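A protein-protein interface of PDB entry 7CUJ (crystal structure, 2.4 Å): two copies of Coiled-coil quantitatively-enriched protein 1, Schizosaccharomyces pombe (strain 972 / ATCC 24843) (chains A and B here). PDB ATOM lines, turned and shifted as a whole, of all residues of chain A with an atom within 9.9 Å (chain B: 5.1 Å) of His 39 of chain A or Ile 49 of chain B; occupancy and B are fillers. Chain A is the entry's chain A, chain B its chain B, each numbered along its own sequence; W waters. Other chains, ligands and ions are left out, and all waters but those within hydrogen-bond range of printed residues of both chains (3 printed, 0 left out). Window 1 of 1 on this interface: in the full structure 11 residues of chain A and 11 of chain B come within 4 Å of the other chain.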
ATOM      1  N   VAL A  30      -4.950 -42.124  29.276  1.00  0.00           N
ATOM      2  CA  VAL A  30      -5.943 -41.617  28.344  1.00  0.00           C
ATOM      3  C   VAL A  30      -7.336 -41.741  28.962  1.00  0.00           C
ATOM      4  O   VAL A  30      -8.162 -40.850  28.800  1.00  0.00           O
ATOM      5  CB  VAL A  30      -5.845 -42.326  26.979  1.00  0.00           C
ATOM      6  CG1 VAL A  30      -7.070 -42.074  26.111  1.00  0.00           C
ATOM      7  CG2 VAL A  30      -4.575 -41.938  26.235  1.00  0.00           C
ATOM      8  N   PHE A  33      -7.942 -39.163  31.525  1.00  0.00           N
ATOM      9  CA  PHE A  33      -8.065 -37.873  30.864  1.00  0.00           C
ATOM     10  C   PHE A  33      -9.155 -37.911  29.789  1.00  0.00           C
ATOM     11  O   PHE A  33      -9.211 -37.022  28.941  1.00  0.00           O
ATOM     12  CB  PHE A  33      -6.726 -37.492  30.218  1.00  0.00           C
ATOM     13  CG  PHE A  33      -5.762 -36.764  31.120  1.00  0.00           C
ATOM     14  CD1 PHE A  33      -4.902 -37.465  31.953  1.00  0.00           C
ATOM     15  CD2 PHE A  33      -5.723 -35.376  31.145  1.00  0.00           C
ATOM     16  CE1 PHE A  33      -4.023 -36.795  32.793  1.00  0.00           C
ATOM     17  CE2 PHE A  33      -4.837 -34.710  31.979  1.00  0.00           C
ATOM     18  CZ  PHE A  33      -3.992 -35.419  32.804  1.00  0.00           C
ATOM     19  N   ALA A  34     -10.024 -38.930  29.823  1.00  0.00           N
ATOM     20  CA  ALA A  34     -10.930 -39.184  28.709  1.00  0.00           C
ATOM     21  C   ALA A  34     -11.782 -37.953  28.395  1.00  0.00           C
ATOM     22  O   ALA A  34     -11.812 -37.513  27.250  1.00  0.00           O
ATOM     23  CB  ALA A  34     -11.767 -40.417  28.954  1.00  0.00           C
ATOM     24  N   PHE A  35     -12.441 -37.398  29.423  1.00  0.00           N
ATOM     25  CA  PHE A  35     -13.303 -36.234  29.280  1.00  0.00           C
ATOM     26  C   PHE A  35     -12.513 -35.061  28.707  1.00  0.00           C
ATOM     27  O   PHE A  35     -12.936 -34.441  27.735  1.00  0.00           O
ATOM     28  CB  PHE A  35     -13.921 -35.830  30.623  1.00  0.00           C
ATOM     29  CG  PHE A  35     -14.864 -34.656  30.536  1.00  0.00           C
ATOM     30  CD1 PHE A  35     -14.385 -33.354  30.516  1.00  0.00           C
ATOM     31  CD2 PHE A  35     -16.234 -34.850  30.442  1.00  0.00           C
ATOM     32  CE1 PHE A  35     -15.251 -32.274  30.414  1.00  0.00           C
ATOM     33  CE2 PHE A  35     -17.103 -33.770  30.346  1.00  0.00           C
ATOM     34  CZ  PHE A  35     -16.612 -32.483  30.336  1.00  0.00           C
ATOM     35  N   CYS A  36     -11.371 -34.776  29.340  1.00  0.00           N
ATOM     36  CA  CYS A  36     -10.502 -33.655  29.026  1.00  0.00           C
ATOM     37  C   CYS A  36      -9.994 -33.733  27.585  1.00  0.00           C
ATOM     38  O   CYS A  36      -9.937 -32.717  26.896  1.00  0.00           O
ATOM     39  CB  CYS A  36      -9.320 -33.639  29.988  1.00  0.00           C
ATOM     40  SG  CYS A  36      -8.360 -32.107  29.926  1.00  0.00           S
ATOM     41  N   ILE A  37      -9.617 -34.939  27.144  1.00  0.00           N
ATOM     42  CA  ILE A  37      -9.096 -35.146  25.802  1.00  0.00           C
ATOM     43  C   ILE A  37     -10.218 -34.911  24.793  1.00  0.00           C
ATOM     44  O   ILE A  37     -10.026 -34.194  23.809  1.00  0.00           O
ATOM     45  CB  ILE A  37      -8.451 -36.543  25.659  1.00  0.00           C
ATOM     46  CG1 ILE A  37      -7.079 -36.603  26.340  1.00  0.00           C
ATOM     47  CG2 ILE A  37      -8.365 -36.961  24.199  1.00  0.00           C
ATOM     48  CD1 ILE A  37      -6.548 -38.004  26.548  1.00  0.00           C
ATOM     49  N   ASP A  38     -11.390 -35.500  25.067  1.00  0.00           N
ATOM     50  CA  ASP A  38     -12.546 -35.386  24.195  1.00  0.00           C
ATOM     51  C   ASP A  38     -12.927 -33.915  24.033  1.00  0.00           C
ATOM     52  O   ASP A  38     -13.216 -33.470  22.925  1.00  0.00           O
ATOM     53  CB  ASP A  38     -13.715 -36.239  24.695  1.00  0.00           C
ATOM     54  CG  ASP A  38     -14.972 -36.093  23.853  1.00  0.00           C
ATOM     55  OD1 ASP A  38     -14.941 -36.500  22.671  1.00  0.00           O
ATOM     56  OD2 ASP A  38     -15.968 -35.561  24.382  1.00  0.00           O
ATOM     57  N   HIS A  39     -12.905 -33.174  25.146  1.00  0.00           N
ATOM     58  CA  HIS A  39     -13.252 -31.762  25.157  1.00  0.00           C
ATOM     59  C   HIS A  39     -12.264 -30.969  24.305  1.00  0.00           C
ATOM     60  O   HIS A  39     -12.669 -30.232  23.408  1.00  0.00           O
ATOM     61  CB  HIS A  39     -13.319 -31.240  26.599  1.00  0.00           C
ATOM     62  CG  HIS A  39     -13.769 -29.822  26.700  1.00  0.00           C
ATOM     63  ND1 HIS A  39     -15.108 -29.476  26.785  1.00  0.00           N
ATOM     64  CD2 HIS A  39     -13.074 -28.664  26.732  1.00  0.00           C
ATOM     65  CE1 HIS A  39     -15.215 -28.166  26.863  1.00  0.00           C
ATOM     66  NE2 HIS A  39     -13.982 -27.643  26.836  1.00  0.00           N
ATOM     67  N   PHE A  40     -10.969 -31.155  24.588  1.00  0.00           N
ATOM     68  CA  PHE A  40      -9.890 -30.389  23.990  1.00  0.00           C
ATOM     69  C   PHE A  40      -9.775 -30.667  22.491  1.00  0.00           C
ATOM     70  O   PHE A  40      -9.425 -29.771  21.723  1.00  0.00           O
ATOM     71  CB  PHE A  40      -8.578 -30.702  24.713  1.00  0.00           C
ATOM     72  CG  PHE A  40      -7.344 -30.114  24.081  1.00  0.00           C
ATOM     73  CD1 PHE A  40      -7.071 -28.757  24.186  1.00  0.00           C
ATOM     74  CD2 PHE A  40      -6.448 -30.919  23.391  1.00  0.00           C
ATOM     75  CE1 PHE A  40      -5.932 -28.215  23.608  1.00  0.00           C
ATOM     76  CE2 PHE A  40      -5.309 -30.377  22.814  1.00  0.00           C
ATOM     77  CZ  PHE A  40      -5.053 -29.026  22.924  1.00  0.00           C
ATOM     78  N   CYS A  41     -10.074 -31.906  22.085  1.00  0.00           N
ATOM     79  CA  CYS A  41      -9.809 -32.347  20.723  1.00  0.00           C
ATOM     80  C   CYS A  41     -11.016 -32.157  19.801  1.00  0.00           C
ATOM     81  O   CYS A  41     -10.909 -32.434  18.608  1.00  0.00           O
ATOM     82  CB  CYS A  41      -9.364 -33.806  20.698  1.00  0.00           C
ATOM     83  SG  CYS A  41      -7.659 -34.057  21.260  1.00  0.00           S
ATOM     84  N   THR A  42     -12.152 -31.680  20.332  1.00  0.00           N
ATOM     85  CA  THR A  42     -13.355 -31.563  19.515  1.00  0.00           C
ATOM     86  C   THR A  42     -13.852 -30.122  19.409  1.00  0.00           C
ATOM     87  O   THR A  42     -14.895 -29.882  18.806  1.00  0.00           O
ATOM     88  CB  THR A  42     -14.497 -32.469  19.999  1.00  0.00           C
ATOM     89  OG1 THR A  42     -14.733 -32.209  21.384  1.00  0.00           O
ATOM     90  CG2 THR A  42     -14.234 -33.941  19.762  1.00  0.00           C
ATOM     91  N   GLY A  43     -13.116 -29.164  19.986  1.00  0.00           N
ATOM     92  CA  GLY A  43     -13.530 -27.773  19.890  1.00  0.00           C
ATOM     93  C   GLY A  43     -12.656 -26.825  20.706  1.00  0.00           C
ATOM     94  O   GLY A  43     -11.712 -27.255  21.365  1.00  0.00           O
ATOM     95  N   PRO A  44     -12.947 -25.501  20.672  1.00  0.00           N
ATOM     96  CA  PRO A  44     -12.251 -24.528  21.515  1.00  0.00           C
ATOM     97  C   PRO A  44     -12.355 -24.903  22.993  1.00  0.00           C
ATOM     98  O   PRO A  44     -13.400 -25.364  23.449  1.00  0.00           O
ATOM     99  CB  PRO A  44     -13.024 -23.221  21.265  1.00  0.00           C
ATOM    100  CG  PRO A  44     -13.636 -23.402  19.893  1.00  0.00           C
ATOM    101  CD  PRO A  44     -13.965 -24.876  19.811  1.00  0.00           C
ATOM    102  N   SER A  45     -11.254 -24.708  23.725  1.00  0.00           N
ATOM    103  CA  SER A  45     -11.186 -25.024  25.142  1.00  0.00           C
ATOM    104  C   SER A  45     -10.568 -23.852  25.901  1.00  0.00           C
ATOM    105  O   SER A  45      -9.808 -23.076  25.331  1.00  0.00           O
ATOM    106  CB  SER A  45     -10.415 -26.299  25.368  1.00  0.00           C
ATOM    107  OG  SER A  45      -9.043 -26.130  25.034  1.00  0.00           O
ATOM    108  N   ASP A  46     -10.894 -23.743  27.194  1.00  0.00           N
ATOM    109  CA  ASP A  46     -10.393 -22.662  28.028  1.00  0.00           C
ATOM    110  C   ASP A  46      -8.945 -22.932  28.435  1.00  0.00           C
ATOM    111  O   ASP A  46      -8.416 -24.015  28.199  1.00  0.00           O
ATOM    112  CB  ASP A  46     -11.317 -22.395  29.222  1.00  0.00           C
ATOM    113  CG  ASP A  46     -11.405 -23.538  30.219  1.00  0.00           C
ATOM    114  OD1 ASP A  46     -10.374 -23.857  30.844  1.00  0.00           O
ATOM    115  OD2 ASP A  46     -12.511 -24.095  30.371  1.00  0.00           O
ATOM    116  N   SER A  47      -8.336 -21.927  29.075  1.00  0.00           N
ATOM    117  CA  SER A  47      -6.938 -21.914  29.475  1.00  0.00           C
ATOM    118  C   SER A  47      -6.617 -23.049  30.448  1.00  0.00           C
ATOM    119  O   SER A  47      -5.527 -23.617  30.397  1.00  0.00           O
ATOM    120  CB  SER A  47      -6.583 -20.568  30.058  1.00  0.00           C
ATOM    121  OG  SER A  47      -5.274 -20.578  30.604  1.00  0.00           O
ATOM    122  N   ARG A  48      -7.569 -23.368  31.334  1.00  0.00           N
ATOM    123  CA  ARG A  48      -7.348 -24.352  32.384  1.00  0.00           C
ATOM    124  C   ARG A  48      -7.417 -25.769  31.816  1.00  0.00           C
ATOM    125  O   ARG A  48      -6.751 -26.667  32.328  1.00  0.00           O
ATOM    126  CB  ARG A  48      -8.309 -24.118  33.554  1.00  0.00           C
ATOM    127  CG  ARG A  48      -7.942 -22.921  34.421  1.00  0.00           C
ATOM    128  CD  ARG A  48      -9.065 -22.457  35.326  1.00  0.00           C
ATOM    129  NE  ARG A  48      -9.459 -23.457  36.307  1.00  0.00           N
ATOM    130  CZ  ARG A  48     -10.648 -24.050  36.359  1.00  0.00           C
ATOM    131  NH1 ARG A  48     -11.591 -23.742  35.482  1.00  0.00           N
ATOM    132  NH2 ARG A  48     -10.892 -24.947  37.296  1.00  0.00           N
ATOM    133  N   ILE A  49      -8.221 -25.960  30.758  1.00  0.00           N
ATOM    134  CA  ILE A  49      -8.275 -27.228  30.045  1.00  0.00           C
ATOM    135  C   ILE A  49      -6.909 -27.485  29.409  1.00  0.00           C
ATOM    136  O   ILE A  49      -6.374 -28.592  29.491  1.00  0.00           O
ATOM    137  CB  ILE A  49      -9.400 -27.238  28.986  1.00  0.00           C
ATOM    138  CG1 ILE A  49     -10.800 -27.191  29.606  1.00  0.00           C
ATOM    139  CG2 ILE A  49      -9.243 -28.417  28.033  1.00  0.00           C
ATOM    140  CD1 ILE A  49     -11.236 -28.467  30.303  1.00  0.00           C
ATOM    141  N   GLN A  50      -6.360 -26.439  28.783  1.00  0.00           N
ATOM    142  CA  GLN A  50      -5.087 -26.498  28.082  1.00  0.00           C
ATOM    143  C   GLN A  50      -3.955 -26.789  29.065  1.00  0.00           C
ATOM    144  O   GLN A  50      -3.006 -27.488  28.720  1.00  0.00           O
ATOM    145  CB  GLN A  50      -4.850 -25.195  27.318  1.00  0.00           C
ATOM    146  CG  GLN A  50      -5.744 -25.047  26.096  1.00  0.00           C
ATOM    147  CD  GLN A  50      -5.801 -23.635  25.567  1.00  0.00           C
ATOM    148  OE1 GLN A  50      -4.966 -22.793  25.889  1.00  0.00           O
ATOM    149  NE2 GLN A  50      -6.796 -23.367  24.737  1.00  0.00           N
ATOM    150  N   LYS A  52      -4.300 -28.580  31.753  1.00  0.00           N
ATOM    151  CA  LYS A  52      -4.455 -29.979  32.117  1.00  0.00           C
ATOM    152  C   LYS A  52      -3.941 -30.887  31.002  1.00  0.00           C
ATOM    153  O   LYS A  52      -3.452 -31.980  31.275  1.00  0.00           O
ATOM    154  CB  LYS A  52      -5.913 -30.277  32.481  1.00  0.00           C
ATOM    155  CG  LYS A  52      -6.259 -30.015  33.940  1.00  0.00           C
ATOM    156  CD  LYS A  52      -7.698 -29.626  34.172  1.00  0.00           C
ATOM    157  CE  LYS A  52      -7.984 -29.343  35.632  1.00  0.00           C
ATOM    158  NZ  LYS A  52      -9.396 -28.947  35.843  1.00  0.00           N
ATOM    159  N   ILE A  53      -4.057 -30.428  29.752  1.00  0.00           N
ATOM    160  CA  ILE A  53      -3.565 -31.195  28.620  1.00  0.00           C
ATOM    161  C   ILE A  53      -2.037 -31.221  28.645  1.00  0.00           C
ATOM    162  O   ILE A  53      -1.436 -32.208  28.229  1.00  0.00           O
ATOM    163  CB  ILE A  53      -4.138 -30.677  27.283  1.00  0.00           C
ATOM    164  CG1 ILE A  53      -5.629 -31.003  27.136  1.00  0.00           C
ATOM    165  CG2 ILE A  53      -3.334 -31.193  26.095  1.00  0.00           C
ATOM    166  CD1 ILE A  53      -5.944 -32.482  27.071  1.00  0.00           C
ATOM    167  N   VAL A 234      -3.473 -30.596  19.420  1.00  0.00           N
ATOM    168  CA  VAL A 234      -4.712 -31.336  19.242  1.00  0.00           C
ATOM    169  C   VAL A 234      -4.425 -32.687  18.583  1.00  0.00           C
ATOM    170  O   VAL A 234      -4.954 -33.710  19.017  1.00  0.00           O
ATOM    171  CB  VAL A 234      -5.765 -30.495  18.488  1.00  0.00           C
ATOM    172  CG1 VAL A 234      -6.873 -31.337  17.875  1.00  0.00           C
ATOM    173  CG2 VAL A 234      -6.360 -29.414  19.381  1.00  0.00           C
ATOM    174  N   VAL A 237      -2.296 -35.304  20.718  1.00  0.00           N
ATOM    175  CA  VAL A 237      -3.132 -35.831  21.788  1.00  0.00           C
ATOM    176  C   VAL A 237      -4.122 -36.831  21.195  1.00  0.00           C
ATOM    177  O   VAL A 237      -4.289 -37.930  21.723  1.00  0.00           O
ATOM    178  CB  VAL A 237      -3.856 -34.717  22.570  1.00  0.00           C
ATOM    179  CG1 VAL A 237      -4.918 -35.280  23.504  1.00  0.00           C
ATOM    180  CG2 VAL A 237      -2.880 -33.844  23.341  1.00  0.00           C
ATOM    181  N   ALA A 241      -4.370 -40.661  22.029  1.00  0.00           N
ATOM    182  CA  ALA A 241      -5.641 -41.097  22.588  1.00  0.00           C
ATOM    183  C   ALA A 241      -6.192 -42.290  21.807  1.00  0.00           C
ATOM    184  O   ALA A 241      -6.591 -43.285  22.407  1.00  0.00           O
ATOM    185  CB  ALA A 241      -6.629 -39.953  22.648  1.00  0.00           C
ATOM    186  N   VAL A 315      -6.896 -35.527  13.962  1.00  0.00           N
ATOM    187  CA  VAL A 315      -8.258 -35.185  14.352  1.00  0.00           C
ATOM    188  C   VAL A 315      -8.632 -33.772  13.898  1.00  0.00           C
ATOM    189  O   VAL A 315      -9.795 -33.392  14.012  1.00  0.00           O
ATOM    190  CB  VAL A 315      -8.510 -35.374  15.864  1.00  0.00           C
ATOM    191  CG1 VAL A 315      -8.394 -36.826  16.304  1.00  0.00           C
ATOM    192  CG2 VAL A 315      -7.628 -34.479  16.720  1.00  0.00           C
ATOM    193  N   CYS B  36     -15.868 -32.431  35.329  1.00  0.00           N
ATOM    194  CA  CYS B  36     -16.580 -31.290  34.777  1.00  0.00           C
ATOM    195  C   CYS B  36     -17.051 -30.364  35.897  1.00  0.00           C
ATOM    196  O   CYS B  36     -16.948 -29.145  35.781  1.00  0.00           O
ATOM    197  CB  CYS B  36     -17.774 -31.781  33.969  1.00  0.00           C
ATOM    198  SG  CYS B  36     -18.565 -30.474  33.002  1.00  0.00           S
ATOM    199  N   HIS B  39     -13.892 -28.717  37.541  1.00  0.00           N
ATOM    200  CA  HIS B  39     -13.401 -27.702  36.623  1.00  0.00           C
ATOM    201  C   HIS B  39     -14.296 -26.463  36.654  1.00  0.00           C
ATOM    202  O   HIS B  39     -13.806 -25.344  36.779  1.00  0.00           O
ATOM    203  CB  HIS B  39     -13.300 -28.283  35.207  1.00  0.00           C
ATOM    204  CG  HIS B  39     -12.733 -27.341  34.201  1.00  0.00           C
ATOM    205  ND1 HIS B  39     -11.372 -27.188  34.019  1.00  0.00           N
ATOM    206  CD2 HIS B  39     -13.332 -26.523  33.309  1.00  0.00           C
ATOM    207  CE1 HIS B  39     -11.153 -26.306  33.063  1.00  0.00           C
ATOM    208  NE2 HIS B  39     -12.343 -25.886  32.608  1.00  0.00           N
ATOM    209  N   PHE B  40     -15.611 -26.681  36.535  1.00  0.00           N
ATOM    210  CA  PHE B  40     -16.567 -25.596  36.400  1.00  0.00           C
ATOM    211  C   PHE B  40     -16.613 -24.742  37.668  1.00  0.00           C
ATOM    212  O   PHE B  40     -16.780 -23.526  37.589  1.00  0.00           O
ATOM    213  CB  PHE B  40     -17.957 -26.142  36.060  1.00  0.00           C
ATOM    214  CG  PHE B  40     -19.020 -25.080  35.966  1.00  0.00           C
ATOM    215  CD1 PHE B  40     -18.966 -24.117  34.969  1.00  0.00           C
ATOM    216  CD2 PHE B  40     -20.069 -25.031  36.874  1.00  0.00           C
ATOM    217  CE1 PHE B  40     -19.936 -23.131  34.878  1.00  0.00           C
ATOM    218  CE2 PHE B  40     -21.040 -24.045  36.779  1.00  0.00           C
ATOM    219  CZ  PHE B  40     -20.971 -23.098  35.783  1.00  0.00           C
ATOM    220  N   SER B  45     -14.475 -21.084  33.051  1.00  0.00           N
ATOM    221  CA  SER B  45     -14.684 -22.197  32.140  1.00  0.00           C
ATOM    222  C   SER B  45     -15.273 -21.683  30.829  1.00  0.00           C
ATOM    223  O   SER B  45     -15.818 -20.585  30.781  1.00  0.00           O
ATOM    224  CB  SER B  45     -15.561 -23.251  32.771  1.00  0.00           C
ATOM    225  OG  SER B  45     -16.819 -22.705  33.145  1.00  0.00           O
ATOM    226  N   ASP B  46     -15.159 -22.497  29.774  1.00  0.00           N
ATOM    227  CA  ASP B  46     -15.599 -22.110  28.444  1.00  0.00           C
ATOM    228  C   ASP B  46     -17.071 -22.468  28.244  1.00  0.00           C
ATOM    229  O   ASP B  46     -17.679 -23.146  29.072  1.00  0.00           O
ATOM    230  CB  ASP B  46     -14.700 -22.708  27.357  1.00  0.00           C
ATOM    231  CG  ASP B  46     -14.700 -24.227  27.311  1.00  0.00           C
ATOM    232  OD1 ASP B  46     -15.788 -24.814  27.145  1.00  0.00           O
ATOM    233  OD2 ASP B  46     -13.606 -24.814  27.433  1.00  0.00           O
ATOM    234  N   SER B  47     -17.609 -22.006  27.108  1.00  0.00           N
ATOM    235  CA  SER B  47     -18.988 -22.192  26.687  1.00  0.00           C
ATOM    236  C   SER B  47     -19.402 -23.661  26.753  1.00  0.00           C
ATOM    237  O   SER B  47     -20.505 -23.971  27.198  1.00  0.00           O
ATOM    238  CB  SER B  47     -19.174 -21.621  25.301  1.00  0.00           C
ATOM    239  OG  SER B  47     -20.219 -22.285  24.608  1.00  0.00           O
ATOM    240  N   ARG B  48     -18.508 -24.554  26.311  1.00  0.00           N
ATOM    241  CA  ARG B  48     -18.833 -25.959  26.105  1.00  0.00           C
ATOM    242  C   ARG B  48     -18.864 -26.721  27.432  1.00  0.00           C
ATOM    243  O   ARG B  48     -19.588 -27.707  27.553  1.00  0.00           O
ATOM    244  CB  ARG B  48     -17.897 -26.582  25.063  1.00  0.00           C
ATOM    245  CG  ARG B  48     -18.291 -26.264  23.627  1.00  0.00           C
ATOM    246  CD  ARG B  48     -17.224 -26.525  22.584  1.00  0.00           C
ATOM    247  NE  ARG B  48     -16.865 -27.934  22.493  1.00  0.00           N
ATOM    248  CZ  ARG B  48     -15.693 -28.445  22.853  1.00  0.00           C
ATOM    249  NH1 ARG B  48     -14.739 -27.660  23.328  1.00  0.00           N
ATOM    250  NH2 ARG B  48     -15.477 -29.743  22.733  1.00  0.00           N
ATOM    251  N   ILE B  49     -18.070 -26.272  28.414  1.00  0.00           N
ATOM    252  CA  ILE B  49     -18.123 -26.839  29.752  1.00  0.00           C
ATOM    253  C   ILE B  49     -19.497 -26.527  30.339  1.00  0.00           C
ATOM    254  O   ILE B  49     -20.172 -27.413  30.856  1.00  0.00           O
ATOM    255  CB  ILE B  49     -16.985 -26.300  30.648  1.00  0.00           C
ATOM    256  CG1 ILE B  49     -15.604 -26.790  30.199  1.00  0.00           C
ATOM    257  CG2 ILE B  49     -17.245 -26.608  32.117  1.00  0.00           C
ATOM    258  CD1 ILE B  49     -15.350 -28.267  30.418  1.00  0.00           C
ATOM    259  N   GLN B  50     -19.891 -25.254  30.221  1.00  0.00           N
ATOM    260  CA  GLN B  50     -21.162 -24.740  30.703  1.00  0.00           C
ATOM    261  C   GLN B  50     -22.320 -25.529  30.094  1.00  0.00           C
ATOM    262  O   GLN B  50     -23.295 -25.825  30.779  1.00  0.00           O
ATOM    263  CB  GLN B  50     -21.282 -23.248  30.384  1.00  0.00           C
ATOM    264  CG  GLN B  50     -20.337 -22.373  31.194  1.00  0.00           C
ATOM    265  CD  GLN B  50     -20.274 -20.944  30.705  1.00  0.00           C
ATOM    266  OE1 GLN B  50     -21.110 -20.492  29.922  1.00  0.00           O
ATOM    267  NE2 GLN B  50     -19.278 -20.213  31.180  1.00  0.00           N
ATOM    268  N   GLU B  51     -22.194 -25.870  28.806  1.00  0.00           N
ATOM    269  CA  GLU B  51     -23.204 -26.626  28.080  1.00  0.00           C
ATOM    270  C   GLU B  51     -23.357 -28.021  28.688  1.00  0.00           C
ATOM    271  O   GLU B  51     -24.473 -28.516  28.828  1.00  0.00           O
ATOM    272  CB  GLU B  51     -22.849 -26.669  26.592  1.00  0.00           C
ATOM    273  CG  GLU B  51     -23.720 -27.602  25.772  1.00  0.00           C
ATOM    274  CD  GLU B  51     -23.315 -27.737  24.312  1.00  0.00           C
ATOM    275  OE1 GLU B  51     -24.223 -27.731  23.454  1.00  0.00           O
ATOM    276  OE2 GLU B  51     -22.094 -27.856  24.034  1.00  0.00           O
ATOM    277  N   LYS B  52     -22.231 -28.646  29.051  1.00  0.00           N
ATOM    278  CA  LYS B  52     -22.254 -29.985  29.620  1.00  0.00           C
ATOM    279  C   LYS B  52     -22.813 -29.944  31.042  1.00  0.00           C
ATOM    280  O   LYS B  52     -23.453 -30.902  31.470  1.00  0.00           O
ATOM    281  CB  LYS B  52     -20.871 -30.638  29.526  1.00  0.00           C
ATOM    282  CG  LYS B  52     -20.538 -31.225  28.162  1.00  0.00           C
ATOM    283  CD  LYS B  52     -19.063 -31.201  27.842  1.00  0.00           C
ATOM    284  CE  LYS B  52     -18.749 -31.745  26.464  1.00  0.00           C
ATOM    285  NZ  LYS B  52     -17.292 -31.712  26.187  1.00  0.00           N
ATOM    286  N   ILE B  53     -22.574 -28.833  31.753  1.00  0.00           N
ATOM    287  CA  ILE B  53     -23.095 -28.635  33.099  1.00  0.00           C
ATOM    288  C   ILE B  53     -24.622 -28.564  33.055  1.00  0.00           C
ATOM    289  O   ILE B  53     -25.282 -29.020  33.984  1.00  0.00           O
ATOM    290  CB  ILE B  53     -22.462 -27.405  33.790  1.00  0.00           C
ATOM    291  CG1 ILE B  53     -21.010 -27.664  34.206  1.00  0.00           C
ATOM    292  CG2 ILE B  53     -23.303 -26.928  34.970  1.00  0.00           C
ATOM    293  CD1 ILE B  53     -20.846 -28.619  35.374  1.00  0.00           C
HETATM  294  O   HOH W   1     -15.966 -34.498  26.904  1.00  0.00           O
HETATM  295  O   HOH W   2     -16.486 -32.494  23.719  1.00  0.00           O
HETATM  296  O   HOH W   3     -11.167 -30.719  36.895  1.00  0.00           O
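NE2 of His 39 of chain A lies within hydrogen-bond range of OD2 of Asp 46 of chain B (2.9 Å).
The backbone carbonyl oxygen of His 39 of chain A sits at hydrogen-bond distance from the guanidinium group of Arg 48 of chain B, at 2.9 Å.
OD2 of Asp 46 of chain A lies within hydrogen-bond range of NE2 of His 39 of chain B, 2.9 Å away.
The backbone carbonyl oxygen (O) of Pro 44 of chain A lies within hydrogen-bond range of the guanidinium group (NH1) of Arg 48 of chain B (2.7 Å).
NH2 of Arg 48 of chain B is in hydrogen-bond range of OG1 of Thr 42 of chain A, at 2.9 Å.
The guanidinium group (NH2) of Arg 48 of chain A is in hydrogen-bond range of the backbone carbonyl oxygen (O) of His 39 of chain B (3.0 Å).
The backbone NH of Asp 46 of chain A sits at hydrogen-bond distance from the side-chain carboxylate of Asp 46 of chain B (2.9 Å).
ND1 of His 39 of chain A is in hydrogen-bond range of NZ of Lys 52 of chain B (3.2 Å).
NZ of Lys 52 of chain A sits at hydrogen-bond distance from ND1 of His 39 of chain B.
The backbone NH (N) of Ile 49 of chain A lies within hydrogen-bond range of the side-chain carboxylate (OD1) of Asp 46 of chain A (3.0 Å).
NE2 of Gln 50 of chain A lies within hydrogen-bond range of O of Ser 45 of chain A (3.1 Å).
The backbone carbonyl oxygen (O) of Asp 38 of chain A sits at hydrogen-bond distance from the side-chain hydroxyl (OG1) of Thr 42 of chain A (2.5 Å).
Phe 35 of chain A touches Cys 36 of chain B.
Phe 35 of chain A touches Lys 52 of chain B.
His 39 of chain A touches Ile 49 of chain B.
Arg 48 of chain B touches Gly 43 of chain A.
Asp 46 of chain B touches Ser 45 of chain A.
Asp 46 of chain A touches Ser 45 of chain B.
CD1 of Ile 49 of chain A touches CE1 of His 39 of chain B, 3.5 Å away.
Of the printed residues of chain B, His 39 of chain A touches Asp 46 (2.9 Å), Arg 48 (2.9 Å), Ile 49 (3.6 Å) and Lys 52 (3.2 Å).
Asp 46 of chain B touches just these residues of chain A: His 39, Ser 45 and Asp 46.
Arg 48 of chain B touches just these residues of chain A: His 39 (2.9 Å), Thr 42 (2.9 Å), Gly 43 (3.5 Å) and Pro 44 (2.7 Å).
Of the printed residues of chain B, Gly 43 of chain A touches Arg 48.
Of the printed residues of chain B, Asp 46 of chain A touches His 39 (2.9 Å), Ser 45 (3.4 Å) and Asp 46 (2.9 Å).
Of the printed residues of chain B, Lys 52 of chain A touches His 39.
Ser 47 of chain A touches none of the printed residues of chain B.
The nearest printed residue of chain B that does not touch Ser 45 of chain A is Arg 48 of chain B (4.6 Å).
Of the 12 printed residues of chain B, 7 touch a printed residue of chain A.
Hydrophobic or aromatic side chains of chain B within 4 Å of the printed part of chain A: His 39 and Ile 49.
Along chain B the printed residues that touch a printed residue of chain A span positions 36 to 52.
Hydrophobic or aromatic side chains of chain A that line the printed part of chain B: Phe 35, His 39 and Ile 49.
Among the printed residues, 16 pairs touch across the chains.
His 39 of chain A touches Ile 49 of chain B, and with the chains exchanged Ile 49 of chain A touches His 39 of chain B.
His 39 of chain A touches Lys 52 of chain B, and with the chains exchanged Lys 52 of chain A touches His 39 of chain B.
Ser 45 of chain A touches Asp 46 of chain B, and with the chains exchanged Asp 46 of chain A touches Ser 45 of chain B.
Positions printed for both chains: 36, 39, 40, 45, 46, 47, 48, 49, 50, 52 and 53.
Water W2 lies within hydrogen-bond range of NZ of Lys 52 of chain B (2.7 Å), OG1 of Thr 42 of chain A (2.9 Å), NH2 of Arg 48 of chain B (3.1 Å) and OD2 of Asp 38 of chain A (3.2 Å).
Water W3 bridges NZ of Lys 52 of chain A (2.7 Å) and N of His 39 of chain B (3.4 Å).
Water W1 lies within hydrogen-bond range of the side-chain carboxylate (OD2) of Asp 38 of chain A (2.7 Å), the backbone carbonyl oxygen (O) of Phe 35 of chain A (3.1 Å) and the side-chain amino group (NZ) of Lys 52 of chain B (3.2 Å).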
